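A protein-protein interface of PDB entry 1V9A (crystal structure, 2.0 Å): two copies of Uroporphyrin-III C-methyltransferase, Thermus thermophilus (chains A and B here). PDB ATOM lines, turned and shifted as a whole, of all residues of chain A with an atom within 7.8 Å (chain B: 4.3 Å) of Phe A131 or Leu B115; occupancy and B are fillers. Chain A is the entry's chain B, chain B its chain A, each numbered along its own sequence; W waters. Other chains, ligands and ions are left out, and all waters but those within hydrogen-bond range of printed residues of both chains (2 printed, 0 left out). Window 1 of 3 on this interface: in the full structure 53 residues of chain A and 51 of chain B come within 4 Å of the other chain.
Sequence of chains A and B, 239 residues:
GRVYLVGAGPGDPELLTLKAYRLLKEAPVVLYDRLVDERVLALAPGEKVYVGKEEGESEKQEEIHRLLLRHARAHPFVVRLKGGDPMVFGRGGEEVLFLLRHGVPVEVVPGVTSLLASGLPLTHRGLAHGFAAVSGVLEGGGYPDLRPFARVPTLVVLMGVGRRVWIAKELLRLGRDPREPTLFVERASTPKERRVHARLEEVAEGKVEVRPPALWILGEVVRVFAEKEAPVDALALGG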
ATOM      1  N   ASP A  85     -27.592 -30.043 -36.924  1.00  0.00           N
ATOM      2  CA  ASP A  85     -26.282 -30.354 -37.505  1.00  0.00           C
ATOM      3  C   ASP A  85     -25.891 -31.688 -36.856  1.00  0.00           C
ATOM      4  O   ASP A  85     -26.019 -31.871 -35.641  1.00  0.00           O
ATOM      5  CB  ASP A  85     -25.243 -29.271 -37.177  1.00  0.00           C
ATOM      6  CG  ASP A  85     -23.846 -29.595 -37.725  1.00  0.00           C
ATOM      7  OD1 ASP A  85     -23.098 -30.383 -37.080  1.00  0.00           O
ATOM      8  OD2 ASP A  85     -23.499 -29.064 -38.806  1.00  0.00           O
ATOM      9  N   MET A  87     -22.967 -33.037 -36.103  1.00  0.00           N
ATOM     10  CA  MET A  87     -21.822 -33.096 -35.197  1.00  0.00           C
ATOM     11  C   MET A  87     -21.923 -32.455 -33.805  1.00  0.00           C
ATOM     12  O   MET A  87     -20.930 -32.367 -33.083  1.00  0.00           O
ATOM     13  CB  MET A  87     -20.580 -32.563 -35.913  1.00  0.00           C
ATOM     14  CG  MET A  87     -20.315 -33.232 -37.247  1.00  0.00           C
ATOM     15  SD  MET A  87     -20.522 -35.044 -37.176  1.00  0.00           S
ATOM     16  CE  MET A  87     -19.177 -35.451 -36.066  1.00  0.00           C
ATOM     17  N   VAL A  88     -23.107 -32.013 -33.411  1.00  0.00           N
ATOM     18  CA  VAL A  88     -23.245 -31.441 -32.082  1.00  0.00           C
ATOM     19  C   VAL A  88     -24.411 -32.055 -31.328  1.00  0.00           C
ATOM     20  O   VAL A  88     -25.556 -32.024 -31.786  1.00  0.00           O
ATOM     21  CB  VAL A  88     -23.403 -29.878 -32.107  1.00  0.00           C
ATOM     22  CG1 VAL A  88     -22.090 -29.225 -32.553  1.00  0.00           C
ATOM     23  CG2 VAL A  88     -24.542 -29.470 -33.022  1.00  0.00           C
ATOM     24  N   PRO A 110     -22.763 -30.595 -42.954  1.00  0.00           N
ATOM     25  CA  PRO A 110     -23.232 -29.698 -41.891  1.00  0.00           C
ATOM     26  C   PRO A 110     -24.645 -29.199 -42.151  1.00  0.00           C
ATOM     27  O   PRO A 110     -25.137 -29.237 -43.283  1.00  0.00           O
ATOM     28  CB  PRO A 110     -22.219 -28.554 -41.922  1.00  0.00           C
ATOM     29  CG  PRO A 110     -20.981 -29.201 -42.453  1.00  0.00           C
ATOM     30  CD  PRO A 110     -21.523 -30.082 -43.556  1.00  0.00           C
ATOM     31  N   THR A 113     -27.928 -25.889 -37.071  1.00  0.00           N
ATOM     32  CA  THR A 113     -28.172 -26.478 -35.747  1.00  0.00           C
ATOM     33  C   THR A 113     -29.333 -25.737 -35.066  1.00  0.00           C
ATOM     34  O   THR A 113     -29.570 -24.559 -35.350  1.00  0.00           O
ATOM     35  CB  THR A 113     -26.910 -26.379 -34.847  1.00  0.00           C
ATOM     36  OG1 THR A 113     -27.216 -26.860 -33.536  1.00  0.00           O
ATOM     37  CG2 THR A 113     -26.436 -24.925 -34.742  1.00  0.00           C
ATOM     38  N   LEU A 115     -29.394 -24.679 -32.224  1.00  0.00           N
ATOM     39  CA  LEU A 115     -28.822 -23.657 -31.345  1.00  0.00           C
ATOM     40  C   LEU A 115     -29.001 -22.282 -31.981  1.00  0.00           C
ATOM     41  O   LEU A 115     -29.028 -21.265 -31.283  1.00  0.00           O
ATOM     42  CB  LEU A 115     -27.323 -23.886 -31.145  1.00  0.00           C
ATOM     43  CG  LEU A 115     -26.857 -25.108 -30.372  1.00  0.00           C
ATOM     44  CD1 LEU A 115     -25.352 -25.246 -30.499  1.00  0.00           C
ATOM     45  CD2 LEU A 115     -27.280 -24.970 -28.927  1.00  0.00           C
ATOM     46  N   LEU A 116     -29.108 -22.276 -33.309  1.00  0.00           N
ATOM     47  CA  LEU A 116     -29.257 -21.057 -34.089  1.00  0.00           C
ATOM     48  C   LEU A 116     -30.645 -20.861 -34.683  1.00  0.00           C
ATOM     49  O   LEU A 116     -30.820 -20.019 -35.547  1.00  0.00           O
ATOM     50  CB  LEU A 116     -28.230 -21.062 -35.218  1.00  0.00           C
ATOM     51  CG  LEU A 116     -26.770 -20.969 -34.754  1.00  0.00           C
ATOM     52  CD1 LEU A 116     -25.827 -21.218 -35.928  1.00  0.00           C
ATOM     53  CD2 LEU A 116     -26.528 -19.595 -34.136  1.00  0.00           C
ATOM     54  N   PRO A 121     -29.690 -12.983 -31.458  1.00  0.00           N
ATOM     55  CA  PRO A 121     -28.247 -12.809 -31.608  1.00  0.00           C
ATOM     56  C   PRO A 121     -27.596 -13.369 -30.343  1.00  0.00           C
ATOM     57  O   PRO A 121     -27.628 -12.728 -29.301  1.00  0.00           O
ATOM     58  CB  PRO A 121     -28.097 -11.292 -31.725  1.00  0.00           C
ATOM     59  CG  PRO A 121     -29.150 -10.794 -30.812  1.00  0.00           C
ATOM     60  CD  PRO A 121     -30.344 -11.705 -31.104  1.00  0.00           C
ATOM     61  N   LEU A 122     -27.019 -14.564 -30.430  1.00  0.00           N
ATOM     62  CA  LEU A 122     -26.367 -15.190 -29.283  1.00  0.00           C
ATOM     63  C   LEU A 122     -25.212 -14.323 -28.792  1.00  0.00           C
ATOM     64  O   LEU A 122     -24.826 -14.390 -27.621  1.00  0.00           O
ATOM     65  CB  LEU A 122     -25.853 -16.594 -29.650  1.00  0.00           C
ATOM     66  CG  LEU A 122     -26.927 -17.552 -30.164  1.00  0.00           C
ATOM     67  CD1 LEU A 122     -26.385 -19.008 -30.154  1.00  0.00           C
ATOM     68  CD2 LEU A 122     -28.159 -17.429 -29.281  1.00  0.00           C
ATOM     69  N   THR A 123     -24.645 -13.541 -29.704  1.00  0.00           N
ATOM     70  CA  THR A 123     -23.573 -12.603 -29.368  1.00  0.00           C
ATOM     71  C   THR A 123     -24.110 -11.217 -29.720  1.00  0.00           C
ATOM     72  O   THR A 123     -24.797 -11.045 -30.721  1.00  0.00           O
ATOM     73  CB  THR A 123     -22.277 -12.820 -30.177  1.00  0.00           C
ATOM     74  OG1 THR A 123     -22.535 -12.609 -31.566  1.00  0.00           O
ATOM     75  CG2 THR A 123     -21.724 -14.230 -29.967  1.00  0.00           C
ATOM     76  N   ALA A 128     -22.872  -9.902 -24.756  1.00  0.00           N
ATOM     77  CA  ALA A 128     -22.154 -11.170 -24.819  1.00  0.00           C
ATOM     78  C   ALA A 128     -21.201 -11.218 -26.001  1.00  0.00           C
ATOM     79  O   ALA A 128     -21.587 -10.944 -27.134  1.00  0.00           O
ATOM     80  CB  ALA A 128     -23.147 -12.321 -24.914  1.00  0.00           C
ATOM     81  N   HIS A 129     -19.950 -11.580 -25.738  1.00  0.00           N
ATOM     82  CA  HIS A 129     -18.969 -11.664 -26.808  1.00  0.00           C
ATOM     83  C   HIS A 129     -18.681 -13.099 -27.184  1.00  0.00           C
ATOM     84  O   HIS A 129     -17.750 -13.376 -27.937  1.00  0.00           O
ATOM     85  CB  HIS A 129     -17.674 -10.962 -26.413  1.00  0.00           C
ATOM     86  CG  HIS A 129     -17.086 -11.440 -25.125  1.00  0.00           C
ATOM     87  ND1 HIS A 129     -17.786 -11.434 -23.935  1.00  0.00           N
ATOM     88  CD2 HIS A 129     -15.849 -11.907 -24.831  1.00  0.00           C
ATOM     89  CE1 HIS A 129     -17.005 -11.877 -22.966  1.00  0.00           C
ATOM     90  NE2 HIS A 129     -15.825 -12.170 -23.483  1.00  0.00           N
ATOM     91  N   GLY A 130     -19.499 -14.009 -26.663  1.00  0.00           N
ATOM     92  CA  GLY A 130     -19.332 -15.417 -26.968  1.00  0.00           C
ATOM     93  C   GLY A 130     -20.498 -16.160 -26.375  1.00  0.00           C
ATOM     94  O   GLY A 130     -21.293 -15.563 -25.667  1.00  0.00           O
ATOM     95  N   PHE A 131     -20.625 -17.451 -26.662  1.00  0.00           N
ATOM     96  CA  PHE A 131     -21.716 -18.211 -26.085  1.00  0.00           C
ATOM     97  C   PHE A 131     -21.243 -19.635 -25.855  1.00  0.00           C
ATOM     98  O   PHE A 131     -20.165 -20.020 -26.299  1.00  0.00           O
ATOM     99  CB  PHE A 131     -22.953 -18.200 -27.005  1.00  0.00           C
ATOM    100  CG  PHE A 131     -22.787 -19.005 -28.273  1.00  0.00           C
ATOM    101  CD1 PHE A 131     -22.218 -18.437 -29.410  1.00  0.00           C
ATOM    102  CD2 PHE A 131     -23.192 -20.337 -28.320  1.00  0.00           C
ATOM    103  CE1 PHE A 131     -22.053 -19.189 -30.584  1.00  0.00           C
ATOM    104  CE2 PHE A 131     -23.032 -21.099 -29.489  1.00  0.00           C
ATOM    105  CZ  PHE A 131     -22.462 -20.523 -30.618  1.00  0.00           C
ATOM    106  N   ALA A 132     -22.044 -20.403 -25.135  1.00  0.00           N
ATOM    107  CA  ALA A 132     -21.719 -21.784 -24.861  1.00  0.00           C
ATOM    108  C   ALA A 132     -23.002 -22.570 -25.021  1.00  0.00           C
ATOM    109  O   ALA A 132     -24.098 -22.014 -24.880  1.00  0.00           O
ATOM    110  CB  ALA A 132     -21.178 -21.930 -23.435  1.00  0.00           C
ATOM    111  N   ALA A 133     -22.854 -23.857 -25.334  1.00  0.00           N
ATOM    112  CA  ALA A 133     -23.974 -24.766 -25.498  1.00  0.00           C
ATOM    113  C   ALA A 133     -23.633 -26.027 -24.695  1.00  0.00           C
ATOM    114  O   ALA A 133     -22.519 -26.539 -24.788  1.00  0.00           O
ATOM    115  CB  ALA A 133     -24.158 -25.108 -26.972  1.00  0.00           C
ATOM    116  N   VAL A 134     -24.585 -26.515 -23.911  1.00  0.00           N
ATOM    117  CA  VAL A 134     -24.354 -27.700 -23.098  1.00  0.00           C
ATOM    118  C   VAL A 134     -25.603 -28.570 -23.014  1.00  0.00           C
ATOM    119  O   VAL A 134     -26.728 -28.074 -23.124  1.00  0.00           O
ATOM    120  CB  VAL A 134     -23.943 -27.304 -21.664  1.00  0.00           C
ATOM    121  CG1 VAL A 134     -25.102 -26.594 -20.974  1.00  0.00           C
ATOM    122  CG2 VAL A 134     -23.521 -28.538 -20.882  1.00  0.00           C
ATOM    123  N   PHE A 149     -19.319 -23.983 -17.718  1.00  0.00           N
ATOM    124  CA  PHE A 149     -20.247 -23.173 -18.515  1.00  0.00           C
ATOM    125  C   PHE A 149     -21.033 -22.114 -17.761  1.00  0.00           C
ATOM    126  O   PHE A 149     -21.504 -21.147 -18.355  1.00  0.00           O
ATOM    127  CB  PHE A 149     -21.276 -24.086 -19.195  1.00  0.00           C
ATOM    128  CG  PHE A 149     -20.669 -25.187 -20.009  1.00  0.00           C
ATOM    129  CD1 PHE A 149     -20.323 -24.977 -21.339  1.00  0.00           C
ATOM    130  CD2 PHE A 149     -20.438 -26.437 -19.441  1.00  0.00           C
ATOM    131  CE1 PHE A 149     -19.755 -25.994 -22.094  1.00  0.00           C
ATOM    132  CE2 PHE A 149     -19.868 -27.459 -20.190  1.00  0.00           C
ATOM    133  CZ  PHE A 149     -19.526 -27.236 -21.523  1.00  0.00           C
ATOM    134  N   VAL A 152     -20.721 -18.120 -18.773  1.00  0.00           N
ATOM    135  CA  VAL A 152     -20.588 -17.589 -20.130  1.00  0.00           C
ATOM    136  C   VAL A 152     -21.778 -16.636 -20.322  1.00  0.00           C
ATOM    137  O   VAL A 152     -22.890 -16.945 -19.923  1.00  0.00           O
ATOM    138  CB  VAL A 152     -20.594 -18.747 -21.158  1.00  0.00           C
ATOM    139  CG1 VAL A 152     -20.435 -18.210 -22.582  1.00  0.00           C
ATOM    140  CG2 VAL A 152     -19.477 -19.711 -20.837  1.00  0.00           C
ATOM    141  N   PRO A 153     -21.545 -15.452 -20.918  1.00  0.00           N
ATOM    142  CA  PRO A 153     -22.567 -14.426 -21.173  1.00  0.00           C
ATOM    143  C   PRO A 153     -23.898 -14.976 -21.691  1.00  0.00           C
ATOM    144  O   PRO A 153     -24.963 -14.697 -21.140  1.00  0.00           O
ATOM    145  CB  PRO A 153     -21.888 -13.507 -22.197  1.00  0.00           C
ATOM    146  CG  PRO A 153     -20.467 -13.632 -21.865  1.00  0.00           C
ATOM    147  CD  PRO A 153     -20.283 -15.097 -21.591  1.00  0.00           C
ATOM    148  N   THR A 154     -23.828 -15.746 -22.771  1.00  0.00           N
ATOM    149  CA  THR A 154     -25.015 -16.354 -23.326  1.00  0.00           C
ATOM    150  C   THR A 154     -24.860 -17.868 -23.208  1.00  0.00           C
ATOM    151  O   THR A 154     -23.908 -18.439 -23.723  1.00  0.00           O
ATOM    152  CB  THR A 154     -25.210 -15.970 -24.798  1.00  0.00           C
ATOM    153  OG1 THR A 154     -25.484 -14.569 -24.888  1.00  0.00           O
ATOM    154  CG2 THR A 154     -26.367 -16.743 -25.400  1.00  0.00           C
ATOM    155  N   LEU A 155     -25.799 -18.509 -22.522  1.00  0.00           N
ATOM    156  CA  LEU A 155     -25.734 -19.956 -22.352  1.00  0.00           C
ATOM    157  C   LEU A 155     -26.927 -20.604 -23.018  1.00  0.00           C
ATOM    158  O   LEU A 155     -28.064 -20.194 -22.793  1.00  0.00           O
ATOM    159  CB  LEU A 155     -25.728 -20.324 -20.857  1.00  0.00           C
ATOM    160  CG  LEU A 155     -25.631 -21.827 -20.533  1.00  0.00           C
ATOM    161  CD1 LEU A 155     -24.364 -22.425 -21.154  1.00  0.00           C
ATOM    162  CD2 LEU A 155     -25.626 -22.014 -19.032  1.00  0.00           C
ATOM    163  N   VAL A 156     -26.670 -21.611 -23.845  1.00  0.00           N
ATOM    164  CA  VAL A 156     -27.750 -22.323 -24.512  1.00  0.00           C
ATOM    165  C   VAL A 156     -27.731 -23.761 -24.000  1.00  0.00           C
ATOM    166  O   VAL A 156     -26.705 -24.416 -24.029  1.00  0.00           O
ATOM    167  CB  VAL A 156     -27.581 -22.321 -26.046  1.00  0.00           C
ATOM    168  CG1 VAL A 156     -28.828 -22.911 -26.691  1.00  0.00           C
ATOM    169  CG2 VAL A 156     -27.350 -20.892 -26.561  1.00  0.00           C
ATOM    170  N   ILE A 217     -32.472 -20.750 -23.895  1.00  0.00           N
ATOM    171  CA  ILE A 217     -31.443 -19.712 -23.920  1.00  0.00           C
ATOM    172  C   ILE A 217     -31.453 -18.788 -22.682  1.00  0.00           C
ATOM    173  O   ILE A 217     -32.491 -18.233 -22.320  1.00  0.00           O
ATOM    174  CB  ILE A 217     -31.564 -18.863 -25.206  1.00  0.00           C
ATOM    175  CG1 ILE A 217     -31.592 -19.783 -26.435  1.00  0.00           C
ATOM    176  CG2 ILE A 217     -30.359 -17.930 -25.335  1.00  0.00           C
ATOM    177  CD1 ILE A 217     -31.835 -19.063 -27.733  1.00  0.00           C
ATOM    178  N   LEU A 218     -30.289 -18.644 -22.043  1.00  0.00           N
ATOM    179  CA  LEU A 218     -30.143 -17.789 -20.864  1.00  0.00           C
ATOM    180  C   LEU A 218     -29.194 -16.616 -21.135  1.00  0.00           C
ATOM    181  O   LEU A 218     -28.098 -16.805 -21.655  1.00  0.00           O
ATOM    182  CB  LEU A 218     -29.602 -18.581 -19.653  1.00  0.00           C
ATOM    183  CG  LEU A 218     -30.434 -19.758 -19.126  1.00  0.00           C
ATOM    184  CD1 LEU A 218     -30.148 -21.013 -19.976  1.00  0.00           C
ATOM    185  CD2 LEU A 218     -30.068 -20.025 -17.661  1.00  0.00           C
ATOM    186  N   VAL A 221     -29.255 -11.205 -24.032  1.00  0.00           N
ATOM    187  CA  VAL A 221     -29.619 -11.195 -25.459  1.00  0.00           C
ATOM    188  C   VAL A 221     -31.091 -11.540 -25.770  1.00  0.00           C
ATOM    189  O   VAL A 221     -31.627 -11.112 -26.788  1.00  0.00           O
ATOM    190  CB  VAL A 221     -28.756 -12.196 -26.302  1.00  0.00           C
ATOM    191  CG1 VAL A 221     -27.288 -11.828 -26.244  1.00  0.00           C
ATOM    192  CG2 VAL A 221     -28.988 -13.643 -25.799  1.00  0.00           C
ATOM    193  N   VAL B  88     -24.302 -14.884 -35.185  1.00  0.00           N
ATOM    194  CA  VAL B  88     -23.197 -15.104 -34.272  1.00  0.00           C
ATOM    195  C   VAL B  88     -21.937 -14.452 -34.818  1.00  0.00           C
ATOM    196  O   VAL B  88     -21.565 -14.660 -35.976  1.00  0.00           O
ATOM    197  CB  VAL B  88     -22.940 -16.620 -33.988  1.00  0.00           C
ATOM    198  CG1 VAL B  88     -23.990 -17.144 -33.004  1.00  0.00           C
ATOM    199  CG2 VAL B  88     -22.971 -17.426 -35.279  1.00  0.00           C
ATOM    200  N   PHE B  89     -21.327 -13.613 -33.984  1.00  0.00           N
ATOM    201  CA  PHE B  89     -20.091 -12.907 -34.308  1.00  0.00           C
ATOM    202  C   PHE B  89     -20.096 -12.026 -35.560  1.00  0.00           C
ATOM    203  O   PHE B  89     -19.042 -11.765 -36.125  1.00  0.00           O
ATOM    204  CB  PHE B  89     -18.947 -13.915 -34.416  1.00  0.00           C
ATOM    205  CG  PHE B  89     -18.828 -14.817 -33.225  1.00  0.00           C
ATOM    206  CD1 PHE B  89     -18.358 -14.329 -32.007  1.00  0.00           C
ATOM    207  CD2 PHE B  89     -19.222 -16.145 -33.309  1.00  0.00           C
ATOM    208  CE1 PHE B  89     -18.283 -15.156 -30.887  1.00  0.00           C
ATOM    209  CE2 PHE B  89     -19.155 -16.974 -32.211  1.00  0.00           C
ATOM    210  CZ  PHE B  89     -18.682 -16.479 -30.989  1.00  0.00           C
ATOM    211  N   THR B 113     -23.081 -22.204 -39.791  1.00  0.00           N
ATOM    212  CA  THR B 113     -22.041 -21.365 -39.215  1.00  0.00           C
ATOM    213  C   THR B 113     -20.655 -21.994 -39.430  1.00  0.00           C
ATOM    214  O   THR B 113     -20.516 -23.216 -39.456  1.00  0.00           O
ATOM    215  CB  THR B 113     -22.294 -21.139 -37.698  1.00  0.00           C
ATOM    216  OG1 THR B 113     -21.198 -20.405 -37.129  1.00  0.00           O
ATOM    217  CG2 THR B 113     -22.451 -22.478 -36.965  1.00  0.00           C
ATOM    218  N   SER B 114     -19.629 -21.170 -39.612  1.00  0.00           N
ATOM    219  CA  SER B 114     -18.300 -21.722 -39.815  1.00  0.00           C
ATOM    220  C   SER B 114     -17.866 -22.538 -38.608  1.00  0.00           C
ATOM    221  O   SER B 114     -16.952 -23.351 -38.711  1.00  0.00           O
ATOM    222  CB  SER B 114     -17.274 -20.621 -40.101  1.00  0.00           C
ATOM    223  OG  SER B 114     -17.082 -19.802 -38.966  1.00  0.00           O
ATOM    224  N   LEU B 115     -18.524 -22.336 -37.466  1.00  0.00           N
ATOM    225  CA  LEU B 115     -18.198 -23.085 -36.252  1.00  0.00           C
ATOM    226  C   LEU B 115     -18.368 -24.592 -36.471  1.00  0.00           C
ATOM    227  O   LEU B 115     -17.746 -25.410 -35.778  1.00  0.00           O
ATOM    228  CB  LEU B 115     -19.128 -22.680 -35.095  1.00  0.00           C
ATOM    229  CG  LEU B 115     -19.039 -21.261 -34.532  1.00  0.00           C
ATOM    230  CD1 LEU B 115     -20.223 -20.980 -33.612  1.00  0.00           C
ATOM    231  CD2 LEU B 115     -17.706 -21.113 -33.783  1.00  0.00           C
ATOM    232  N   LEU B 116     -19.226 -24.943 -37.427  1.00  0.00           N
ATOM    233  CA  LEU B 116     -19.541 -26.340 -37.724  1.00  0.00           C
ATOM    234  C   LEU B 116     -19.032 -26.783 -39.078  1.00  0.00           C
ATOM    235  O   LEU B 116     -19.403 -27.860 -39.555  1.00  0.00           O
ATOM    236  CB  LEU B 116     -21.057 -26.543 -37.698  1.00  0.00           C
ATOM    237  CG  LEU B 116     -21.818 -26.134 -36.435  1.00  0.00           C
ATOM    238  CD1 LEU B 116     -23.329 -26.273 -36.657  1.00  0.00           C
ATOM    239  CD2 LEU B 116     -21.359 -26.992 -35.273  1.00  0.00           C
ATOM    240  N   ALA B 117     -18.190 -25.963 -39.698  1.00  0.00           N
ATOM    241  CA  ALA B 117     -17.681 -26.272 -41.024  1.00  0.00           C
ATOM    242  C   ALA B 117     -16.511 -27.248 -41.086  1.00  0.00           C
ATOM    243  O   ALA B 117     -16.099 -27.621 -42.183  1.00  0.00           O
ATOM    244  CB  ALA B 117     -17.309 -24.979 -41.749  1.00  0.00           C
ATOM    245  N   LEU B 122     -17.910 -31.562 -31.965  1.00  0.00           N
ATOM    246  CA  LEU B 122     -17.554 -30.590 -30.926  1.00  0.00           C
ATOM    247  C   LEU B 122     -17.942 -31.152 -29.578  1.00  0.00           C
ATOM    248  O   LEU B 122     -17.464 -30.704 -28.536  1.00  0.00           O
ATOM    249  CB  LEU B 122     -18.267 -29.249 -31.167  1.00  0.00           C
ATOM    250  CG  LEU B 122     -17.942 -28.563 -32.497  1.00  0.00           C
ATOM    251  CD1 LEU B 122     -18.636 -27.206 -32.551  1.00  0.00           C
ATOM    252  CD2 LEU B 122     -16.429 -28.393 -32.642  1.00  0.00           C
ATOM    253  N   ALA B 132     -18.017 -24.103 -26.357  1.00  0.00           N
ATOM    254  CA  ALA B 132     -18.164 -22.652 -26.281  1.00  0.00           C
ATOM    255  C   ALA B 132     -17.517 -22.041 -27.490  1.00  0.00           C
ATOM    256  O   ALA B 132     -16.615 -22.631 -28.092  1.00  0.00           O
ATOM    257  CB  ALA B 132     -17.514 -22.103 -25.010  1.00  0.00           C
ATOM    258  N   ALA B 133     -17.992 -20.858 -27.854  1.00  0.00           N
ATOM    259  CA  ALA B 133     -17.447 -20.150 -28.992  1.00  0.00           C
ATOM    260  C   ALA B 133     -17.225 -18.703 -28.570  1.00  0.00           C
ATOM    261  O   ALA B 133     -18.093 -18.081 -27.951  1.00  0.00           O
ATOM    262  CB  ALA B 133     -18.419 -20.208 -30.168  1.00  0.00           C
ATOM    263  N   PHE B 149     -14.736 -18.496 -20.520  1.00  0.00           N
ATOM    264  CA  PHE B 149     -14.604 -19.584 -21.489  1.00  0.00           C
ATOM    265  C   PHE B 149     -13.372 -20.459 -21.324  1.00  0.00           C
ATOM    266  O   PHE B 149     -13.233 -21.492 -21.992  1.00  0.00           O
ATOM    267  CB  PHE B 149     -14.555 -19.038 -22.921  1.00  0.00           C
ATOM    268  CG  PHE B 149     -15.652 -18.078 -23.258  1.00  0.00           C
ATOM    269  CD1 PHE B 149     -15.594 -16.756 -22.822  1.00  0.00           C
ATOM    270  CD2 PHE B 149     -16.739 -18.492 -24.023  1.00  0.00           C
ATOM    271  CE1 PHE B 149     -16.608 -15.849 -23.146  1.00  0.00           C
ATOM    272  CE2 PHE B 149     -17.762 -17.599 -24.354  1.00  0.00           C
ATOM    273  CZ  PHE B 149     -17.696 -16.270 -23.913  1.00  0.00           C
ATOM    274  N   VAL B 156     -14.105 -23.060 -29.185  1.00  0.00           N
ATOM    275  CA  VAL B 156     -13.904 -22.703 -30.568  1.00  0.00           C
ATOM    276  C   VAL B 156     -13.708 -21.198 -30.611  1.00  0.00           C
ATOM    277  O   VAL B 156     -14.500 -20.432 -30.055  1.00  0.00           O
ATOM    278  CB  VAL B 156     -15.094 -23.118 -31.436  1.00  0.00           C
ATOM    279  CG1 VAL B 156     -14.776 -22.845 -32.913  1.00  0.00           C
ATOM    280  CG2 VAL B 156     -15.396 -24.609 -31.215  1.00  0.00           C
ATOM    281  N   LEU B 158     -13.135 -17.816 -32.990  1.00  0.00           N
ATOM    282  CA  LEU B 158     -13.303 -17.227 -34.312  1.00  0.00           C
ATOM    283  C   LEU B 158     -12.532 -15.908 -34.299  1.00  0.00           C
ATOM    284  O   LEU B 158     -12.317 -15.328 -33.233  1.00  0.00           O
ATOM    285  CB  LEU B 158     -14.788 -16.973 -34.619  1.00  0.00           C
ATOM    286  CG  LEU B 158     -15.686 -18.218 -34.766  1.00  0.00           C
ATOM    287  CD1 LEU B 158     -17.007 -17.810 -35.424  1.00  0.00           C
ATOM    288  CD2 LEU B 158     -15.004 -19.264 -35.633  1.00  0.00           C
ATOM    289  N   LEU B 215     -10.781 -21.204 -38.370  1.00  0.00           N
ATOM    290  CA  LEU B 215     -11.567 -21.694 -37.266  1.00  0.00           C
ATOM    291  C   LEU B 215     -10.557 -22.308 -36.309  1.00  0.00           C
ATOM    292  O   LEU B 215      -9.704 -23.074 -36.733  1.00  0.00           O
ATOM    293  CB  LEU B 215     -12.485 -22.765 -37.822  1.00  0.00           C
ATOM    294  CG  LEU B 215     -13.572 -23.441 -37.020  1.00  0.00           C
ATOM    295  CD1 LEU B 215     -14.579 -22.407 -36.547  1.00  0.00           C
ATOM    296  CD2 LEU B 215     -14.231 -24.477 -37.925  1.00  0.00           C
HETATM  297  O   HOH W   1     -25.407 -24.039 -38.282  1.00  0.00           O
HETATM  298  O   HOH W   2     -20.610 -29.978 -38.325  1.00  0.00           O
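Pro A110 touches Leu B116 (CG to O, 3.6 Å). Thr A113 touches Leu B116. Leu A116 touches Val B88. Thr B113 touches Leu A116. CG1 of Val B88 touches CB of Leu A122, at 3.9 Å. Gly A130 touches Ala B133. Phe A131 touches Phe B89 (CE1 to CE2, 3.99 Å). Phe A131 touches Ala B132 (O to CA, 3.3 Å). Phe A131 touches Phe B149 (N to CE2, 3.7 Å). Pro A153 touches Phe B149.
Printed residues of chain B that touch a printed residue of chain A: Val B88, Phe B89, Thr B113, Leu B115, Leu B116, Leu B122, Ala B132, Ala B133 and Phe B149. Hydrophobic or aromatic side chains of chain B that line the printed part of chain A: Val B88, Phe B89, Leu B115, Leu B116, Ala B132, Ala B133 and Phe B149. Along chain B the printed residues that touch a printed residue of chain A span positions 88 to 149. Of the 26 printed residues of chain A, 14 touch a printed residue of chain B. Among the printed residues, no Asp or Glu carboxylate lies within 4 Å of a Lys or Arg side-chain nitrogen of the other chain.
Water W2 lies within hydrogen-bond range of the backbone carbonyl oxygen of Leu B116 (2.7 Å) and the side-chain carboxylate of Asp A85 (2.8 Å). Water W1 lies within hydrogen-bond range of the backbone NH (N) of Thr B113 and the backbone NH (N) of Thr A113.
O of Ala A132 is in hydrogen-bond range of N of Val A156 (2.8 Å). The backbone NH of Ala A132 sits at hydrogen-bond distance from the backbone carbonyl oxygen of Thr A154 (3.1 Å). The backbone carbonyl oxygen (O) of Leu A122 lies within hydrogen-bond range of the side-chain hydroxyl (OG1) of Thr A154 (2.8 Å). The side-chain hydroxyl (OG1) of Thr A113 lies close to the backbone NH (N) of Leu A115 (3.3 Å). OD1 of Asp A85 lies within hydrogen-bond range of N of Met A87 (2.8 Å). N of Val B156 is in hydrogen-bond range of O of Ala B132.
The backbone NH of Leu B122 is in hydrogen-bond range of the backbone carbonyl oxygen of Met A87 (3.3 Å). N of Ala B133 is in hydrogen-bond range of O of Phe A131, 2.8 Å away. OG1 of Thr A123 sits at hydrogen-bond distance from N of Phe B89, 2.9 Å away.
Of the printed residues of chain B, Met A87 touches Leu B122. Of the printed residues of chain B, Phe A131 touches Val B88 (3.7 Å), Phe B89 (3.99 Å), Leu B115 (3.8 Å), Ala B132 (3.3 Å), Ala B133 (2.8 Å) and Phe B149 (3.7 Å). Printed residues of chain B within 4 Å of Pro A153: Phe B149 (3.7 Å). Of the printed residues of chain A, Phe B89 touches Thr A123, His A129 and Phe A131. No residue of chain A comes within 4 Å of Ser B114. Leu B115 touches one residue of chain A. Of the printed residues of chain A, Leu B116 touches Asp A85, Val A88, Pro A110 and Thr A113. Ala B117 touches none of the printed residues of chain A. The nearest printed residue of chain B that does not touch Phe A131 is Thr B113 (6.6 Å). The nearest residue of chain A that does not touch Leu B115 is Leu A116 (6.1 Å).
Val A88 touches Leu B116, and with the chains exchanged Leu A116 touches Val B88. Thr A113 touches Leu B116, and with the chains exchanged Leu A116 touches Thr B113. Leu A122 touches Val B88, but with the chains exchanged Val A88 does not touch Leu B122 (4.001 Å). Ala B132 touches its own counterpart, Ala A132. Positions printed for both chains: 88, 113, 115, 116, 122, 132, 133, 149 and 156.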
